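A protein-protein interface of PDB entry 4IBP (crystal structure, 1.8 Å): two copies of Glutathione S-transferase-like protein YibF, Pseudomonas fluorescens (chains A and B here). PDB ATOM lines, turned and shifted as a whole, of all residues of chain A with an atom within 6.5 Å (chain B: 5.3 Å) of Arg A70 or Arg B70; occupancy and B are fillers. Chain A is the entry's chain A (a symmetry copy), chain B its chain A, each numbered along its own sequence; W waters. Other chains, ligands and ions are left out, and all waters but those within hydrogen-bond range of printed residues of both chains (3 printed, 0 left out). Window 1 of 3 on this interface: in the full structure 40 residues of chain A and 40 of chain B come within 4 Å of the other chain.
Asp A68 touches Arg B70, and with the chains exchanged Arg A70 touches Asp B68. Asp A68 touches Ala B101, and with the chains exchanged Ala A101 touches Asp B68. Arg A70 touches its own counterpart, Arg B70. Of the 7 pairs that touch across the chains among the printed residues, 5 have their exchanged pair printed and touching as well.
Of the printed residues of chain B, Asp A68 touches Arg B70 and Ala B101. Printed residues of chain B within 4 Å of Arg A70: Asp B68 (2.5 Å) and Arg B70 (3.8 Å). Of the printed residues of chain B, Leu A97 touches Val B71 (3.8 Å). Of the printed residues of chain B, Ala A101 touches Asp B68. Of the printed residues of chain A, Arg B70 touches Asp A68 (2.5 Å) and Arg A70 (3.8 Å). Of the printed residues of chain A, Val B71 touches Leu A97 (3.8 Å). The nearest printed residue of chain B that does not touch Arg A70 is Val B71 (4.01 Å).
Printed residues of chain B that touch a printed residue of chain A: Asp B68, Arg B70, Val B71 and Ala B101. Hydrophobic or aromatic side chains of chain B within 4 Å of the printed part of chain A: Val B71 and Ala B101.
NH2 of Arg B70 is in salt-bridge range of OD2 of Asp A68 (2.5 Å). OD2 of Asp B68 is in salt-bridge range of NH2 of Arg A70 (2.5 Å).
Among the printed residues, pairs that only touch across the chains: Tyr A67 with Ala B101 (3.4 Å), Asp A68 with Ala B101 (3.7 Å), Arg A70 with Arg B70 (3.8 Å), Leu A97 with Val B71 (3.8 Å) and Ala A101 with Asp B68 (3.7 Å).
The guanidinium group of Arg B70 is in salt-bridge range of the side-chain carboxylate of Asp B104 (2.9 Å). The guanidinium group (NE) of Arg A70 is in salt-bridge range of the side-chain carboxylate (OD2) of Asp A104.
Water W2 lies within hydrogen-bond range of the backbone carbonyl oxygen (O) of Ala B101 (2.7 Å) and the side-chain carboxylate (OD2) of Asp A68 (3.3 Å). Water W3 bridges the backbone carbonyl oxygen of Ala A101 (2.8 Å) and the side-chain carboxylate of Asp B68 (3.3 Å). Water W1 bridges NH2 of Arg B70 (2.9 Å) and NH2 of Arg A70 (2.9 Å).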
ATOM      1  N   LYS A  16      13.119   2.906  15.656  1.00  0.00           N
ATOM      2  CA  LYS A  16      11.821   3.376  15.164  1.00  0.00           C
ATOM      3  C   LYS A  16      11.988   4.671  14.375  1.00  0.00           C
ATOM      4  O   LYS A  16      11.406   4.821  13.304  1.00  0.00           O
ATOM      5  CB  LYS A  16      10.821   3.651  16.303  1.00  0.00           C
ATOM      6  CG  LYS A  16      10.410   2.461  17.139  1.00  0.00           C
ATOM      7  CD  LYS A  16       9.243   2.837  18.079  1.00  0.00           C
ATOM      8  CE  LYS A  16       9.678   3.850  19.108  1.00  0.00           C
ATOM      9  NZ  LYS A  16       8.526   4.208  20.008  1.00  0.00           N
ATOM     10  N   VAL A  17      12.732   5.626  14.939  1.00  0.00           N
ATOM     11  CA  VAL A  17      12.974   6.885  14.256  1.00  0.00           C
ATOM     12  C   VAL A  17      13.754   6.702  12.926  1.00  0.00           C
ATOM     13  O   VAL A  17      13.411   7.322  11.921  1.00  0.00           O
ATOM     14  CB  VAL A  17      13.678   7.901  15.170  1.00  0.00           C
ATOM     15  CG1 VAL A  17      13.986   9.176  14.413  1.00  0.00           C
ATOM     16  CG2 VAL A  17      12.827   8.186  16.417  1.00  0.00           C
ATOM     17  N   PRO A  56      16.096   8.040  21.678  1.00  0.00           N
ATOM     18  CA  PRO A  56      16.532   9.162  20.841  1.00  0.00           C
ATOM     19  C   PRO A  56      16.203  10.513  21.440  1.00  0.00           C
ATOM     20  O   PRO A  56      15.298  10.622  22.275  1.00  0.00           O
ATOM     21  CB  PRO A  56      15.693   8.988  19.579  1.00  0.00           C
ATOM     22  CG  PRO A  56      14.391   8.398  20.113  1.00  0.00           C
ATOM     23  CD  PRO A  56      14.869   7.405  21.152  1.00  0.00           C
ATOM     24  N   TYR A  67      11.905  15.147  22.518  1.00  0.00           N
ATOM     25  CA  TYR A  67      11.951  13.763  22.997  1.00  0.00           C
ATOM     26  C   TYR A  67      10.568  13.506  23.593  1.00  0.00           C
ATOM     27  O   TYR A  67       9.831  14.468  23.799  1.00  0.00           O
ATOM     28  CB  TYR A  67      13.073  13.585  24.032  1.00  0.00           C
ATOM     29  CG  TYR A  67      13.070  14.663  25.093  1.00  0.00           C
ATOM     30  CD1 TYR A  67      12.316  14.523  26.239  1.00  0.00           C
ATOM     31  CD2 TYR A  67      13.824  15.827  24.934  1.00  0.00           C
ATOM     32  CE1 TYR A  67      12.299  15.522  27.228  1.00  0.00           C
ATOM     33  CE2 TYR A  67      13.816  16.830  25.922  1.00  0.00           C
ATOM     34  CZ  TYR A  67      13.050  16.659  27.053  1.00  0.00           C
ATOM     35  OH  TYR A  67      13.026  17.638  28.026  1.00  0.00           O
ATOM     36  N   ASP A  68      10.162  12.257  23.849  1.00  0.00           N
ATOM     37  CA  ASP A  68      10.904  11.028  23.590  1.00  0.00           C
ATOM     38  C   ASP A  68      10.586  10.525  22.188  1.00  0.00           C
ATOM     39  O   ASP A  68      10.140  11.308  21.344  1.00  0.00           O
ATOM     40  CB  ASP A  68      10.519   9.976  24.641  1.00  0.00           C
ATOM     41  CG  ASP A  68       9.011   9.687  24.670  1.00  0.00           C
ATOM     42  OD1 ASP A  68       8.239  10.340  23.946  1.00  0.00           O
ATOM     43  OD2 ASP A  68       8.586   8.811  25.440  1.00  0.00           O
ATOM     44  N   SER A  69      10.793   9.237  21.933  1.00  0.00           N
ATOM     45  CA  SER A  69      10.649   8.698  20.576  1.00  0.00           C
ATOM     46  C   SER A  69       9.276   8.971  19.953  1.00  0.00           C
ATOM     47  O   SER A  69       9.174   9.342  18.779  1.00  0.00           O
ATOM     48  CB  SER A  69      10.962   7.192  20.541  1.00  0.00           C
ATOM     49  OG  SER A  69      10.073   6.438  21.351  1.00  0.00           O
ATOM     50  N   ARG A  70       8.213   8.784  20.728  1.00  0.00           N
ATOM     51  CA  ARG A  70       6.872   8.991  20.186  1.00  0.00           C
ATOM     52  C   ARG A  70       6.622  10.437  19.764  1.00  0.00           C
ATOM     53  O   ARG A  70       5.921  10.677  18.772  1.00  0.00           O
ATOM     54  CB  ARG A  70       5.801   8.512  21.161  1.00  0.00           C
ATOM     55  CG  ARG A  70       5.687   7.004  21.235  1.00  0.00           C
ATOM     56  CD  ARG A  70       4.483   6.636  22.071  1.00  0.00           C
ATOM     57  NE  ARG A  70       4.839   6.300  23.445  1.00  0.00           N
ATOM     58  CZ  ARG A  70       3.957   5.954  24.372  1.00  0.00           C
ATOM     59  NH1 ARG A  70       2.666   5.922  24.074  1.00  0.00           N
ATOM     60  NH2 ARG A  70       4.365   5.653  25.594  1.00  0.00           N
ATOM     61  N   VAL A  71       7.178  11.394  20.506  1.00  0.00           N
ATOM     62  CA  VAL A  71       7.084  12.806  20.130  1.00  0.00           C
ATOM     63  C   VAL A  71       7.886  13.073  18.840  1.00  0.00           C
ATOM     64  O   VAL A  71       7.425  13.764  17.932  1.00  0.00           O
ATOM     65  CB  VAL A  71       7.585  13.724  21.264  1.00  0.00           C
ATOM     66  CG1 VAL A  71       7.436  15.187  20.869  1.00  0.00           C
ATOM     67  CG2 VAL A  71       6.824  13.441  22.555  1.00  0.00           C
ATOM     68  N   ILE A  72       9.081  12.499  18.766  1.00  0.00           N
ATOM     69  CA  ILE A  72       9.929  12.640  17.591  1.00  0.00           C
ATOM     70  C   ILE A  72       9.233  12.025  16.363  1.00  0.00           C
ATOM     71  O   ILE A  72       9.240  12.618  15.276  1.00  0.00           O
ATOM     72  CB  ILE A  72      11.295  11.989  17.831  1.00  0.00           C
ATOM     73  CG1 ILE A  72      12.089  12.778  18.874  1.00  0.00           C
ATOM     74  CG2 ILE A  72      12.090  11.861  16.529  1.00  0.00           C
ATOM     75  CD1 ILE A  72      13.221  11.954  19.508  1.00  0.00           C
ATOM     76  N   LEU A  73       8.632  10.849  16.538  1.00  0.00           N
ATOM     77  CA  LEU A  73       7.935  10.177  15.430  1.00  0.00           C
ATOM     78  C   LEU A  73       6.775  11.036  14.914  1.00  0.00           C
ATOM     79  O   LEU A  73       6.582  11.179  13.710  1.00  0.00           O
ATOM     80  CB  LEU A  73       7.451   8.806  15.878  1.00  0.00           C
ATOM     81  CG  LEU A  73       8.603   7.834  16.142  1.00  0.00           C
ATOM     82  CD1 LEU A  73       8.110   6.640  16.962  1.00  0.00           C
ATOM     83  CD2 LEU A  73       9.218   7.342  14.820  1.00  0.00           C
ATOM     84  N   ASP A  74       6.027  11.642  15.831  1.00  0.00           N
ATOM     85  CA  ASP A  74       4.893  12.472  15.451  1.00  0.00           C
ATOM     86  C   ASP A  74       5.392  13.689  14.672  1.00  0.00           C
ATOM     87  O   ASP A  74       4.838  14.040  13.626  1.00  0.00           O
ATOM     88  CB  ASP A  74       4.115  12.925  16.696  1.00  0.00           C
ATOM     89  CG  ASP A  74       2.827  13.672  16.347  1.00  0.00           C
ATOM     90  OD1 ASP A  74       2.702  14.851  16.713  1.00  0.00           O
ATOM     91  OD2 ASP A  74       1.952  13.088  15.683  1.00  0.00           O
ATOM     92  N   TYR A  75       6.457  14.308  15.164  1.00  0.00           N
ATOM     93  CA  TYR A  75       7.049  15.461  14.477  1.00  0.00           C
ATOM     94  C   TYR A  75       7.473  15.112  13.046  1.00  0.00           C
ATOM     95  O   TYR A  75       7.099  15.776  12.078  1.00  0.00           O
ATOM     96  CB  TYR A  75       8.262  15.954  15.251  1.00  0.00           C
ATOM     97  CG  TYR A  75       9.039  17.021  14.528  1.00  0.00           C
ATOM     98  CD1 TYR A  75       8.577  18.335  14.467  1.00  0.00           C
ATOM     99  CD2 TYR A  75      10.245  16.715  13.918  1.00  0.00           C
ATOM    100  CE1 TYR A  75       9.303  19.319  13.804  1.00  0.00           C
ATOM    101  CE2 TYR A  75      10.983  17.688  13.248  1.00  0.00           C
ATOM    102  CZ  TYR A  75      10.506  18.982  13.197  1.00  0.00           C
ATOM    103  OH  TYR A  75      11.238  19.939  12.530  1.00  0.00           O
ATOM    104  N   ILE A  86       1.104   8.041  10.809  1.00  0.00           N
ATOM    105  CA  ILE A  86       0.172   8.066  11.932  1.00  0.00           C
ATOM    106  C   ILE A  86      -1.156   8.649  11.455  1.00  0.00           C
ATOM    107  O   ILE A  86      -1.201   9.789  10.977  1.00  0.00           O
ATOM    108  CB  ILE A  86       0.676   8.963  13.088  1.00  0.00           C
ATOM    109  CG1 ILE A  86       2.060   8.519  13.569  1.00  0.00           C
ATOM    110  CG2 ILE A  86      -0.328   8.958  14.237  1.00  0.00           C
ATOM    111  CD1 ILE A  86       2.769   9.536  14.494  1.00  0.00           C
ATOM    112  N   LEU A  97      -2.223   3.923  17.366  1.00  0.00           N
ATOM    113  CA  LEU A  97      -1.370   4.475  18.416  1.00  0.00           C
ATOM    114  C   LEU A  97      -1.291   3.538  19.635  1.00  0.00           C
ATOM    115  O   LEU A  97      -0.274   3.480  20.330  1.00  0.00           O
ATOM    116  CB  LEU A  97      -1.862   5.881  18.835  1.00  0.00           C
ATOM    117  CG  LEU A  97      -1.464   6.973  17.830  1.00  0.00           C
ATOM    118  CD1 LEU A  97      -1.861   8.373  18.329  1.00  0.00           C
ATOM    119  CD2 LEU A  97       0.032   6.929  17.549  1.00  0.00           C
ATOM    120  N   ALA A 100       1.116   0.790  18.751  1.00  0.00           N
ATOM    121  CA  ALA A 100       2.465   1.331  18.899  1.00  0.00           C
ATOM    122  C   ALA A 100       2.862   1.397  20.377  1.00  0.00           C
ATOM    123  O   ALA A 100       4.013   1.130  20.736  1.00  0.00           O
ATOM    124  CB  ALA A 100       2.571   2.708  18.220  1.00  0.00           C
ATOM    125  N   ALA A 101       1.908   1.757  21.238  1.00  0.00           N
ATOM    126  CA  ALA A 101       2.170   1.806  22.675  1.00  0.00           C
ATOM    127  C   ALA A 101       2.402   0.413  23.267  1.00  0.00           C
ATOM    128  O   ALA A 101       3.134   0.258  24.246  1.00  0.00           O
ATOM    129  CB  ALA A 101       1.039   2.540  23.427  1.00  0.00           C
ATOM    130  N   ASP A 104       5.924  -0.253  22.372  1.00  0.00           N
ATOM    131  CA  ASP A 104       6.768   0.484  23.308  1.00  0.00           C
ATOM    132  C   ASP A 104       6.838  -0.205  24.673  1.00  0.00           C
ATOM    133  O   ASP A 104       7.893  -0.226  25.298  1.00  0.00           O
ATOM    134  CB  ASP A 104       6.294   1.940  23.485  1.00  0.00           C
ATOM    135  CG  ASP A 104       6.604   2.809  22.277  1.00  0.00           C
ATOM    136  OD1 ASP A 104       7.308   2.342  21.357  1.00  0.00           O
ATOM    137  OD2 ASP A 104       6.155   3.974  22.248  1.00  0.00           O
ATOM    138  N   ASP A 108      10.000  -1.378  26.685  1.00  0.00           N
ATOM    139  CA  ASP A 108      10.231  -0.891  28.047  1.00  0.00           C
ATOM    140  C   ASP A 108      10.626  -2.050  28.961  1.00  0.00           C
ATOM    141  O   ASP A 108      11.588  -1.962  29.720  1.00  0.00           O
ATOM    142  CB  ASP A 108       8.976  -0.225  28.626  1.00  0.00           C
ATOM    143  CG  ASP A 108       8.592   1.081  27.921  1.00  0.00           C
ATOM    144  OD1 ASP A 108       9.403   1.640  27.153  1.00  0.00           O
ATOM    145  OD2 ASP A 108       7.459   1.559  28.159  1.00  0.00           O
ATOM    146  N   ILE A 158       3.051   3.590  11.728  1.00  0.00           N
ATOM    147  CA  ILE A 158       3.558   3.746  13.086  1.00  0.00           C
ATOM    148  C   ILE A 158       3.452   2.455  13.928  1.00  0.00           C
ATOM    149  O   ILE A 158       4.370   2.125  14.690  1.00  0.00           O
ATOM    150  CB  ILE A 158       2.878   4.948  13.808  1.00  0.00           C
ATOM    151  CG1 ILE A 158       3.554   5.208  15.149  1.00  0.00           C
ATOM    152  CG2 ILE A 158       1.390   4.703  13.983  1.00  0.00           C
ATOM    153  CD1 ILE A 158       4.991   5.697  15.011  1.00  0.00           C
ATOM    154  N   SER A 162       6.785   0.189  15.024  1.00  0.00           N
ATOM    155  CA  SER A 162       7.080  -0.010  16.432  1.00  0.00           C
ATOM    156  C   SER A 162       7.139  -1.495  16.804  1.00  0.00           C
ATOM    157  O   SER A 162       8.067  -1.917  17.491  1.00  0.00           O
ATOM    158  CB  SER A 162       6.066   0.728  17.311  1.00  0.00           C
ATOM    159  OG  SER A 162       6.056   2.114  17.003  1.00  0.00           O
ATOM    160  N   LYS B  16      -3.213  12.236  35.496  1.00  0.00           N
ATOM    161  CA  LYS B  16      -3.239  13.064  34.287  1.00  0.00           C
ATOM    162  C   LYS B  16      -4.578  12.917  33.571  1.00  0.00           C
ATOM    163  O   LYS B  16      -5.163  13.910  33.145  1.00  0.00           O
ATOM    164  CB  LYS B  16      -2.133  12.684  33.285  1.00  0.00           C
ATOM    165  CG  LYS B  16      -0.708  12.881  33.751  1.00  0.00           C
ATOM    166  CD  LYS B  16       0.277  12.683  32.576  1.00  0.00           C
ATOM    167  CE  LYS B  16       0.265  11.256  32.091  1.00  0.00           C
ATOM    168  NZ  LYS B  16       1.225  11.087  30.944  1.00  0.00           N
ATOM    169  N   ASP B  68      -1.142   3.754  26.164  1.00  0.00           N
ATOM    170  CA  ASP B  68      -0.990   4.107  27.571  1.00  0.00           C
ATOM    171  C   ASP B  68      -1.573   5.493  27.817  1.00  0.00           C
ATOM    172  O   ASP B  68      -2.400   5.956  27.026  1.00  0.00           O
ATOM    173  CB  ASP B  68       0.500   4.075  27.940  1.00  0.00           C
ATOM    174  CG  ASP B  68       1.350   5.009  27.066  1.00  0.00           C
ATOM    175  OD1 ASP B  68       0.825   5.627  26.124  1.00  0.00           O
ATOM    176  OD2 ASP B  68       2.564   5.113  27.308  1.00  0.00           O
ATOM    177  N   SER B  69      -1.147   6.160  28.884  1.00  0.00           N
ATOM    178  CA  SER B  69      -1.756   7.436  29.275  1.00  0.00           C
ATOM    179  C   SER B  69      -1.736   8.489  28.161  1.00  0.00           C
ATOM    180  O   SER B  69      -2.727   9.189  27.931  1.00  0.00           O
ATOM    181  CB  SER B  69      -1.103   7.996  30.550  1.00  0.00           C
ATOM    182  OG  SER B  69       0.280   8.266  30.374  1.00  0.00           O
ATOM    183  N   ARG B  70      -0.609   8.613  27.469  1.00  0.00           N
ATOM    184  CA  ARG B  70      -0.509   9.623  26.417  1.00  0.00           C
ATOM    185  C   ARG B  70      -1.483   9.376  25.267  1.00  0.00           C
ATOM    186  O   ARG B  70      -2.006  10.336  24.686  1.00  0.00           O
ATOM    187  CB  ARG B  70       0.922   9.748  25.904  1.00  0.00           C
ATOM    188  CG  ARG B  70       1.845  10.464  26.868  1.00  0.00           C
ATOM    189  CD  ARG B  70       3.177  10.707  26.196  1.00  0.00           C
ATOM    190  NE  ARG B  70       4.177   9.713  26.565  1.00  0.00           N
ATOM    191  CZ  ARG B  70       5.419   9.708  26.098  1.00  0.00           C
ATOM    192  NH1 ARG B  70       5.799  10.632  25.228  1.00  0.00           N
ATOM    193  NH2 ARG B  70       6.270   8.774  26.493  1.00  0.00           N
ATOM    194  N   VAL B  71      -1.723   8.109  24.930  1.00  0.00           N
ATOM    195  CA  VAL B  71      -2.715   7.761  23.912  1.00  0.00           C
ATOM    196  C   VAL B  71      -4.136   8.101  24.408  1.00  0.00           C
ATOM    197  O   VAL B  71      -4.952   8.661  23.677  1.00  0.00           O
ATOM    198  CB  VAL B  71      -2.630   6.269  23.530  1.00  0.00           C
ATOM    199  CG1 VAL B  71      -3.639   5.942  22.438  1.00  0.00           C
ATOM    200  CG2 VAL B  71      -1.218   5.915  23.074  1.00  0.00           C
ATOM    201  N   ILE B  72      -4.409   7.772  25.665  1.00  0.00           N
ATOM    202  CA  ILE B  72      -5.700   8.064  26.272  1.00  0.00           C
ATOM    203  C   ILE B  72      -5.929   9.587  26.311  1.00  0.00           C
ATOM    204  O   ILE B  72      -7.028  10.064  25.996  1.00  0.00           O
ATOM    205  CB  ILE B  72      -5.784   7.460  27.677  1.00  0.00           C
ATOM    206  CG1 ILE B  72      -5.825   5.933  27.602  1.00  0.00           C
ATOM    207  CG2 ILE B  72      -6.996   7.996  28.444  1.00  0.00           C
ATOM    208  CD1 ILE B  72      -5.430   5.261  28.927  1.00  0.00           C
ATOM    209  N   LEU B  73      -4.898  10.342  26.688  1.00  0.00           N
ATOM    210  CA  LEU B  73      -5.011  11.806  26.756  1.00  0.00           C
ATOM    211  C   LEU B  73      -5.328  12.395  25.376  1.00  0.00           C
ATOM    212  O   LEU B  73      -6.176  13.272  25.243  1.00  0.00           O
ATOM    213  CB  LEU B  73      -3.732  12.399  27.329  1.00  0.00           C
ATOM    214  CG  LEU B  73      -3.530  12.044  28.804  1.00  0.00           C
ATOM    215  CD1 LEU B  73      -2.078  12.298  29.215  1.00  0.00           C
ATOM    216  CD2 LEU B  73      -4.478  12.862  29.699  1.00  0.00           C
ATOM    217  N   ASP B  74      -4.671  11.878  24.343  1.00  0.00           N
ATOM    218  CA  ASP B  74      -4.886  12.370  22.990  1.00  0.00           C
ATOM    219  C   ASP B  74      -6.324  12.074  22.564  1.00  0.00           C
ATOM    220  O   ASP B  74      -7.012  12.939  22.015  1.00  0.00           O
ATOM    221  CB  ASP B  74      -3.900  11.713  22.013  1.00  0.00           C
ATOM    222  CG  ASP B  74      -3.980  12.306  20.606  1.00  0.00           C
ATOM    223  OD1 ASP B  74      -4.304  11.567  19.663  1.00  0.00           O
ATOM    224  OD2 ASP B  74      -3.745  13.517  20.448  1.00  0.00           O
ATOM    225  N   TYR B  75      -6.785  10.862  22.847  1.00  0.00           N
ATOM    226  CA  TYR B  75      -8.164  10.480  22.524  1.00  0.00           C
ATOM    227  C   TYR B  75      -9.181  11.411  23.193  1.00  0.00           C
ATOM    228  O   TYR B  75     -10.064  11.978  22.547  1.00  0.00           O
ATOM    229  CB  TYR B  75      -8.422   9.051  22.977  1.00  0.00           C
ATOM    230  CG  TYR B  75      -9.862   8.634  22.848  1.00  0.00           C
ATOM    231  CD1 TYR B  75     -10.413   8.313  21.608  1.00  0.00           C
ATOM    232  CD2 TYR B  75     -10.667   8.548  23.972  1.00  0.00           C
ATOM    233  CE1 TYR B  75     -11.743   7.921  21.496  1.00  0.00           C
ATOM    234  CE2 TYR B  75     -12.002   8.159  23.876  1.00  0.00           C
ATOM    235  CZ  TYR B  75     -12.528   7.848  22.639  1.00  0.00           C
ATOM    236  OH  TYR B  75     -13.848   7.469  22.550  1.00  0.00           O
ATOM    237  N   ALA B 101       6.381  14.969  27.838  1.00  0.00           N
ATOM    238  CA  ALA B 101       7.260  13.802  27.866  1.00  0.00           C
ATOM    239  C   ALA B 101       8.335  13.914  28.951  1.00  0.00           C
ATOM    240  O   ALA B 101       8.789  12.907  29.496  1.00  0.00           O
ATOM    241  CB  ALA B 101       7.901  13.549  26.484  1.00  0.00           C
ATOM    242  N   ASP B 104       6.489  12.938  31.999  1.00  0.00           N
ATOM    243  CA  ASP B 104       6.378  11.482  32.005  1.00  0.00           C
ATOM    244  C   ASP B 104       7.693  10.815  32.417  1.00  0.00           C
ATOM    245  O   ASP B 104       7.679   9.816  33.128  1.00  0.00           O
ATOM    246  CB  ASP B 104       5.926  10.935  30.636  1.00  0.00           C
ATOM    247  CG  ASP B 104       4.455  11.203  30.356  1.00  0.00           C
ATOM    248  OD1 ASP B 104       3.740  11.680  31.262  1.00  0.00           O
ATOM    249  OD2 ASP B 104       4.003  10.921  29.227  1.00  0.00           O
HETATM  250  O   HOH W   1       6.472   6.083  27.526  1.00  0.00           O
HETATM  251  O   HOH W   2       9.170  10.471  28.279  1.00  0.00           O
HETATM  252  O   HOH W   3       3.422   2.039  26.322  1.00  0.00           O
